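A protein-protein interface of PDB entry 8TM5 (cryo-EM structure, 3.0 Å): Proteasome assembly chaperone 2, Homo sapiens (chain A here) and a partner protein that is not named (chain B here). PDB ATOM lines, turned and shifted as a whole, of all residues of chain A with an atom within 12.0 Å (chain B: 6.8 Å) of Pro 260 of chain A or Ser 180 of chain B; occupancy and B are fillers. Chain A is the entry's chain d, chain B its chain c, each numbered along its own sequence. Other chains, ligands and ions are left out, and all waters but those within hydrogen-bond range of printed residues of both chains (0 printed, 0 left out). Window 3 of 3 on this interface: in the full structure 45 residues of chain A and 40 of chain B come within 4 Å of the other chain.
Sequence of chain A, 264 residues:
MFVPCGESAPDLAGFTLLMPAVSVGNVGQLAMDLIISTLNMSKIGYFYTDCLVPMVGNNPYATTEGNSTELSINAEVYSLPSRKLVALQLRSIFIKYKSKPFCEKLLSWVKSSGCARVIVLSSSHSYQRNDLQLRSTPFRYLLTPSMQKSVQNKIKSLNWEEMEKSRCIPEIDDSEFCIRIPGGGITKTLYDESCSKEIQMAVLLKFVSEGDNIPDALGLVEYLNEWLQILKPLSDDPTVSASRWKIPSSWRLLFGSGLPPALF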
ATOM      1  N   ARG A 252     -15.092   0.225 -21.582  1.00  0.00           N
ATOM      2  CA  ARG A 252     -15.276   1.668 -21.560  1.00  0.00           C
ATOM      3  C   ARG A 252     -16.131   2.060 -22.753  1.00  0.00           C
ATOM      4  O   ARG A 252     -16.075   1.417 -23.805  1.00  0.00           O
ATOM      5  CB  ARG A 252     -13.930   2.400 -21.609  1.00  0.00           C
ATOM      6  CG  ARG A 252     -13.941   3.796 -21.020  1.00  0.00           C
ATOM      7  CD  ARG A 252     -12.529   4.351 -20.930  1.00  0.00           C
ATOM      8  NE  ARG A 252     -11.922   4.509 -22.247  1.00  0.00           N
ATOM      9  CZ  ARG A 252     -12.098   5.558 -23.039  1.00  0.00           C
ATOM     10  NH1 ARG A 252     -12.871   6.572 -22.687  1.00  0.00           N
ATOM     11  NH2 ARG A 252     -11.484   5.589 -24.219  1.00  0.00           N
ATOM     12  N   LEU A 253     -16.917   3.119 -22.580  1.00  0.00           N
ATOM     13  CA  LEU A 253     -17.759   3.645 -23.651  1.00  0.00           C
ATOM     14  C   LEU A 253     -18.621   2.537 -24.250  1.00  0.00           C
ATOM     15  O   LEU A 253     -18.788   2.430 -25.467  1.00  0.00           O
ATOM     16  CB  LEU A 253     -16.910   4.313 -24.732  1.00  0.00           C
ATOM     17  CG  LEU A 253     -15.749   5.184 -24.253  1.00  0.00           C
ATOM     18  CD1 LEU A 253     -14.996   5.759 -25.441  1.00  0.00           C
ATOM     19  CD2 LEU A 253     -16.246   6.293 -23.344  1.00  0.00           C
ATOM     20  N   PHE A 255     -21.639   2.240 -24.396  1.00  0.00           N
ATOM     21  CA  PHE A 255     -22.876   2.710 -25.005  1.00  0.00           C
ATOM     22  C   PHE A 255     -22.584   3.760 -26.070  1.00  0.00           C
ATOM     23  O   PHE A 255     -23.417   4.635 -26.332  1.00  0.00           O
ATOM     24  CB  PHE A 255     -23.833   3.274 -23.956  1.00  0.00           C
ATOM     25  CG  PHE A 255     -24.580   2.222 -23.188  1.00  0.00           C
ATOM     26  CD1 PHE A 255     -24.058   1.692 -22.021  1.00  0.00           C
ATOM     27  CD2 PHE A 255     -25.808   1.765 -23.634  1.00  0.00           C
ATOM     28  CE1 PHE A 255     -24.746   0.725 -21.316  1.00  0.00           C
ATOM     29  CE2 PHE A 255     -26.499   0.799 -22.932  1.00  0.00           C
ATOM     30  CZ  PHE A 255     -25.968   0.279 -21.772  1.00  0.00           C
ATOM     31  N   GLY A 256     -21.409   3.687 -26.689  1.00  0.00           N
ATOM     32  CA  GLY A 256     -21.038   4.624 -27.729  1.00  0.00           C
ATOM     33  C   GLY A 256     -20.337   5.858 -27.201  1.00  0.00           C
ATOM     34  O   GLY A 256     -19.803   5.855 -26.089  1.00  0.00           O
ATOM     35  N   SER A 257     -20.338   6.923 -27.996  1.00  0.00           N
ATOM     36  CA  SER A 257     -19.673   8.165 -27.631  1.00  0.00           C
ATOM     37  C   SER A 257     -20.529   8.917 -26.613  1.00  0.00           C
ATOM     38  O   SER A 257     -21.530   8.405 -26.105  1.00  0.00           O
ATOM     39  CB  SER A 257     -19.410   9.004 -28.877  1.00  0.00           C
ATOM     40  OG  SER A 257     -18.423   8.407 -29.696  1.00  0.00           O
ATOM     41  N   GLY A 258     -20.138  10.151 -26.302  1.00  0.00           N
ATOM     42  CA  GLY A 258     -20.940  10.991 -25.443  1.00  0.00           C
ATOM     43  C   GLY A 258     -22.138  11.564 -26.174  1.00  0.00           C
ATOM     44  O   GLY A 258     -22.344  11.336 -27.366  1.00  0.00           O
ATOM     45  N   LEU A 259     -22.935  12.323 -25.443  1.00  0.00           N
ATOM     46  CA  LEU A 259     -24.150  12.894 -25.996  1.00  0.00           C
ATOM     47  C   LEU A 259     -23.906  14.316 -26.483  1.00  0.00           C
ATOM     48  O   LEU A 259     -23.039  15.025 -25.964  1.00  0.00           O
ATOM     49  CB  LEU A 259     -25.268  12.872 -24.946  1.00  0.00           C
ATOM     50  CG  LEU A 259     -25.088  13.746 -23.703  1.00  0.00           C
ATOM     51  CD1 LEU A 259     -25.561  15.168 -23.941  1.00  0.00           C
ATOM     52  CD2 LEU A 259     -25.823  13.130 -22.524  1.00  0.00           C
ATOM     53  N   PRO A 260     -24.657  14.769 -27.485  1.00  0.00           N
ATOM     54  CA  PRO A 260     -24.368  16.068 -28.104  1.00  0.00           C
ATOM     55  C   PRO A 260     -24.711  17.215 -27.171  1.00  0.00           C
ATOM     56  O   PRO A 260     -25.592  17.083 -26.308  1.00  0.00           O
ATOM     57  CB  PRO A 260     -25.261  16.079 -29.357  1.00  0.00           C
ATOM     58  CG  PRO A 260     -25.964  14.743 -29.389  1.00  0.00           C
ATOM     59  CD  PRO A 260     -25.898  14.184 -28.016  1.00  0.00           C
ATOM     60  N   PRO A 261     -24.045  18.363 -27.315  1.00  0.00           N
ATOM     61  CA  PRO A 261     -24.355  19.492 -26.421  1.00  0.00           C
ATOM     62  C   PRO A 261     -25.709  20.121 -26.694  1.00  0.00           C
ATOM     63  O   PRO A 261     -26.381  20.563 -25.754  1.00  0.00           O
ATOM     64  CB  PRO A 261     -23.206  20.472 -26.690  1.00  0.00           C
ATOM     65  CG  PRO A 261     -22.744  20.153 -28.067  1.00  0.00           C
ATOM     66  CD  PRO A 261     -22.967  18.683 -28.266  1.00  0.00           C
ATOM     67  N   ALA A 262     -26.131  20.177 -27.959  1.00  0.00           N
ATOM     68  CA  ALA A 262     -27.402  20.812 -28.290  1.00  0.00           C
ATOM     69  C   ALA A 262     -28.553  20.148 -27.545  1.00  0.00           C
ATOM     70  O   ALA A 262     -29.375  20.821 -26.914  1.00  0.00           O
ATOM     71  CB  ALA A 262     -27.634  20.758 -29.800  1.00  0.00           C
ATOM     72  N   LEU A 263     -28.626  18.823 -27.609  1.00  0.00           N
ATOM     73  CA  LEU A 263     -29.633  18.080 -26.869  1.00  0.00           C
ATOM     74  C   LEU A 263     -29.362  18.179 -25.375  1.00  0.00           C
ATOM     75  O   LEU A 263     -28.231  18.416 -24.940  1.00  0.00           O
ATOM     76  CB  LEU A 263     -29.643  16.613 -27.303  1.00  0.00           C
ATOM     77  CG  LEU A 263     -30.899  15.776 -27.048  1.00  0.00           C
ATOM     78  CD1 LEU A 263     -32.167  16.541 -27.392  1.00  0.00           C
ATOM     79  CD2 LEU A 263     -30.825  14.475 -27.829  1.00  0.00           C
ATOM     80  N   PHE A 264     -30.415  18.003 -24.584  1.00  0.00           N
ATOM     81  CA  PHE A 264     -30.287  18.073 -23.135  1.00  0.00           C
ATOM     82  C   PHE A 264     -29.779  19.440 -22.693  1.00  0.00           C
ATOM     83  O   PHE A 264     -28.682  19.558 -22.148  1.00  0.00           O
ATOM     84  CB  PHE A 264     -29.350  16.975 -22.623  1.00  0.00           C
ATOM     85  CG  PHE A 264     -29.775  15.586 -23.007  1.00  0.00           C
ATOM     86  CD1 PHE A 264     -30.749  14.922 -22.284  1.00  0.00           C
ATOM     87  CD2 PHE A 264     -29.194  14.940 -24.084  1.00  0.00           C
ATOM     88  CE1 PHE A 264     -31.140  13.648 -22.627  1.00  0.00           C
ATOM     89  CE2 PHE A 264     -29.583  13.663 -24.434  1.00  0.00           C
ATOM     90  CZ  PHE A 264     -30.558  13.017 -23.704  1.00  0.00           C
ATOM     91  N   VAL B 172     -15.970   9.896 -38.224  1.00  0.00           N
ATOM     92  CA  VAL B 172     -15.734  10.281 -36.835  1.00  0.00           C
ATOM     93  C   VAL B 172     -16.828   9.719 -35.938  1.00  0.00           C
ATOM     94  O   VAL B 172     -16.629   9.538 -34.730  1.00  0.00           O
ATOM     95  CB  VAL B 172     -15.633  11.812 -36.712  1.00  0.00           C
ATOM     96  CG1 VAL B 172     -15.493  12.218 -35.256  1.00  0.00           C
ATOM     97  CG2 VAL B 172     -14.450  12.333 -37.515  1.00  0.00           C
ATOM     98  N   THR B 177     -15.405   8.272 -27.902  1.00  0.00           N
ATOM     99  CA  THR B 177     -14.660   9.174 -27.038  1.00  0.00           C
ATOM    100  C   THR B 177     -15.516   9.515 -25.828  1.00  0.00           C
ATOM    101  O   THR B 177     -16.737   9.341 -25.846  1.00  0.00           O
ATOM    102  CB  THR B 177     -14.255  10.454 -27.777  1.00  0.00           C
ATOM    103  OG1 THR B 177     -13.622  11.359 -26.862  1.00  0.00           O
ATOM    104  CG2 THR B 177     -15.473  11.130 -28.396  1.00  0.00           C
ATOM    105  N   SER B 178     -14.857  10.004 -24.777  1.00  0.00           N
ATOM    106  CA  SER B 178     -15.574  10.376 -23.563  1.00  0.00           C
ATOM    107  C   SER B 178     -16.580  11.485 -23.838  1.00  0.00           C
ATOM    108  O   SER B 178     -17.708  11.453 -23.332  1.00  0.00           O
ATOM    109  CB  SER B 178     -14.583  10.810 -22.484  1.00  0.00           C
ATOM    110  OG  SER B 178     -13.702  11.806 -22.974  1.00  0.00           O
ATOM    111  N   GLU B 179     -16.194  12.472 -24.640  1.00  0.00           N
ATOM    112  CA  GLU B 179     -17.051  13.600 -24.960  1.00  0.00           C
ATOM    113  C   GLU B 179     -17.868  13.286 -26.210  1.00  0.00           C
ATOM    114  O   GLU B 179     -17.812  12.185 -26.763  1.00  0.00           O
ATOM    115  CB  GLU B 179     -16.224  14.878 -25.146  1.00  0.00           C
ATOM    116  CG  GLU B 179     -14.924  14.696 -25.915  1.00  0.00           C
ATOM    117  CD  GLU B 179     -14.206  16.007 -26.161  1.00  0.00           C
ATOM    118  OE1 GLU B 179     -14.026  16.777 -25.193  1.00  0.00           O
ATOM    119  OE2 GLU B 179     -13.822  16.269 -27.319  1.00  0.00           O
ATOM    120  N   SER B 180     -18.641  14.271 -26.660  1.00  0.00           N
ATOM    121  CA  SER B 180     -19.499  14.076 -27.821  1.00  0.00           C
ATOM    122  C   SER B 180     -18.664  13.783 -29.059  1.00  0.00           C
ATOM    123  O   SER B 180     -17.569  14.323 -29.242  1.00  0.00           O
ATOM    124  CB  SER B 180     -20.364  15.314 -28.057  1.00  0.00           C
ATOM    125  OG  SER B 180     -21.245  15.113 -29.149  1.00  0.00           O
ATOM    126  N   THR B 181     -19.197  12.914 -29.921  1.00  0.00           N
ATOM    127  CA  THR B 181     -18.508  12.569 -31.157  1.00  0.00           C
ATOM    128  C   THR B 181     -18.479  13.726 -32.146  1.00  0.00           C
ATOM    129  O   THR B 181     -17.751  13.656 -33.142  1.00  0.00           O
ATOM    130  CB  THR B 181     -19.169  11.354 -31.808  1.00  0.00           C
ATOM    131  OG1 THR B 181     -18.341  10.867 -32.871  1.00  0.00           O
ATOM    132  CG2 THR B 181     -20.541  11.717 -32.358  1.00  0.00           C
ATOM    133  N   GLY B 182     -19.258  14.777 -31.904  1.00  0.00           N
ATOM    134  CA  GLY B 182     -19.249  15.943 -32.764  1.00  0.00           C
ATOM    135  C   GLY B 182     -18.355  17.045 -32.236  1.00  0.00           C
ATOM    136  O   GLY B 182     -18.457  18.196 -32.671  1.00  0.00           O
ATOM    137  N   SER B 183     -17.475  16.706 -31.298  1.00  0.00           N
ATOM    138  CA  SER B 183     -16.594  17.665 -30.639  1.00  0.00           C
ATOM    139  C   SER B 183     -15.140  17.245 -30.795  1.00  0.00           C
ATOM    140  O   SER B 183     -14.314  17.420 -29.897  1.00  0.00           O
ATOM    141  CB  SER B 183     -16.960  17.805 -29.165  1.00  0.00           C
ATOM    142  OG  SER B 183     -16.824  16.567 -28.489  1.00  0.00           O
ATOM    143  N   LEU B 184     -14.811  16.681 -31.945  1.00  0.00           N
ATOM    144  CA  LEU B 184     -13.462  16.276 -32.295  1.00  0.00           C
ATOM    145  C   LEU B 184     -12.932  17.121 -33.443  1.00  0.00           C
ATOM    146  O   LEU B 184     -13.701  17.721 -34.201  1.00  0.00           O
ATOM    147  CB  LEU B 184     -13.431  14.795 -32.695  1.00  0.00           C
ATOM    148  CG  LEU B 184     -13.794  13.730 -31.654  1.00  0.00           C
ATOM    149  CD1 LEU B 184     -13.220  14.055 -30.282  1.00  0.00           C
ATOM    150  CD2 LEU B 184     -15.295  13.538 -31.578  1.00  0.00           C
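Of the 12 printed residues of chain A, 5 touch a printed residue of chain B. Printed residues of chain A that touch a printed residue of chain B: Leu 253, Ser 257, Gly 258, Leu 259 and Pro 260. Of the 9 printed residues of chain B, 5 touch a printed residue of chain A. Among the printed residues, 9 pairs touch across the chains.
Of the printed residues of chain B, Ser 257 of chain A touches Thr 177 and Thr 181. Of the printed residues of chain B, Gly 258 of chain A touches Thr 177 (3.5 Å), Ser 178 (3.9 Å), Glu 179 (3.1 Å) and Ser 180 (3.98 Å). Of chain A, only Leu 253 (3.5 Å), Ser 257 (3.5 Å) and Gly 258 (3.5 Å) come within 4 Å of Thr 177 of chain B. Of chain A, only Gly 258 (3.98 Å), Leu 259 (3.4 Å) and Pro 260 (3.4 Å) come within 4 Å of Ser 180 of chain B. No residue of chain A comes within 4 Å of Gly 182 of chain B. Ser 183 of chain B touches none of the printed residues of chain A. No residue of chain A comes within 4 Å of Leu 184 of chain B. The nearest residue of chain A that does not touch Ser 180 of chain B is Pro 261 of chain A (4.1 Å).
Among the printed residues, merely in contact across the chains: Leu 259 of chain A with Ser 180 of chain B, Pro 260 of chain A with Ser 180 of chain B, Ser 257 of chain A with Thr 177 of chain B, Gly 258 of chain A with Thr 177 of chain B, Leu 253 of chain A with Thr 177 of chain B, Ser 257 of chain A with Thr 181 of chain B, Gly 258 of chain A with Ser 178 of chain B and Gly 258 of chain A with Ser 180 of chain B.
The backbone carbonyl oxygen (O) of Ser 180 of chain B is in hydrogen-bond range of the side-chain hydroxyl (OG) of Ser 183 of chain B. The side-chain carboxylate of Glu 179 of chain B is in hydrogen-bond range of the side-chain hydroxyl of Ser 183 of chain B, at 3.2 Å. The side-chain hydroxyl (OG) of Ser 180 of chain B lies close to the backbone NH (N) of Gly 182 of chain B (3.4 Å). The backbone carbonyl oxygen (O) of Val 172 of chain B is in hydrogen-bond range of the side-chain hydroxyl (OG1) of Thr 181 of chain B (2.9 Å).
The backbone carbonyl oxygen (O) of Glu 179 of chain B sits at hydrogen-bond distance from the backbone NH (N) of Gly 258 of chain A.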
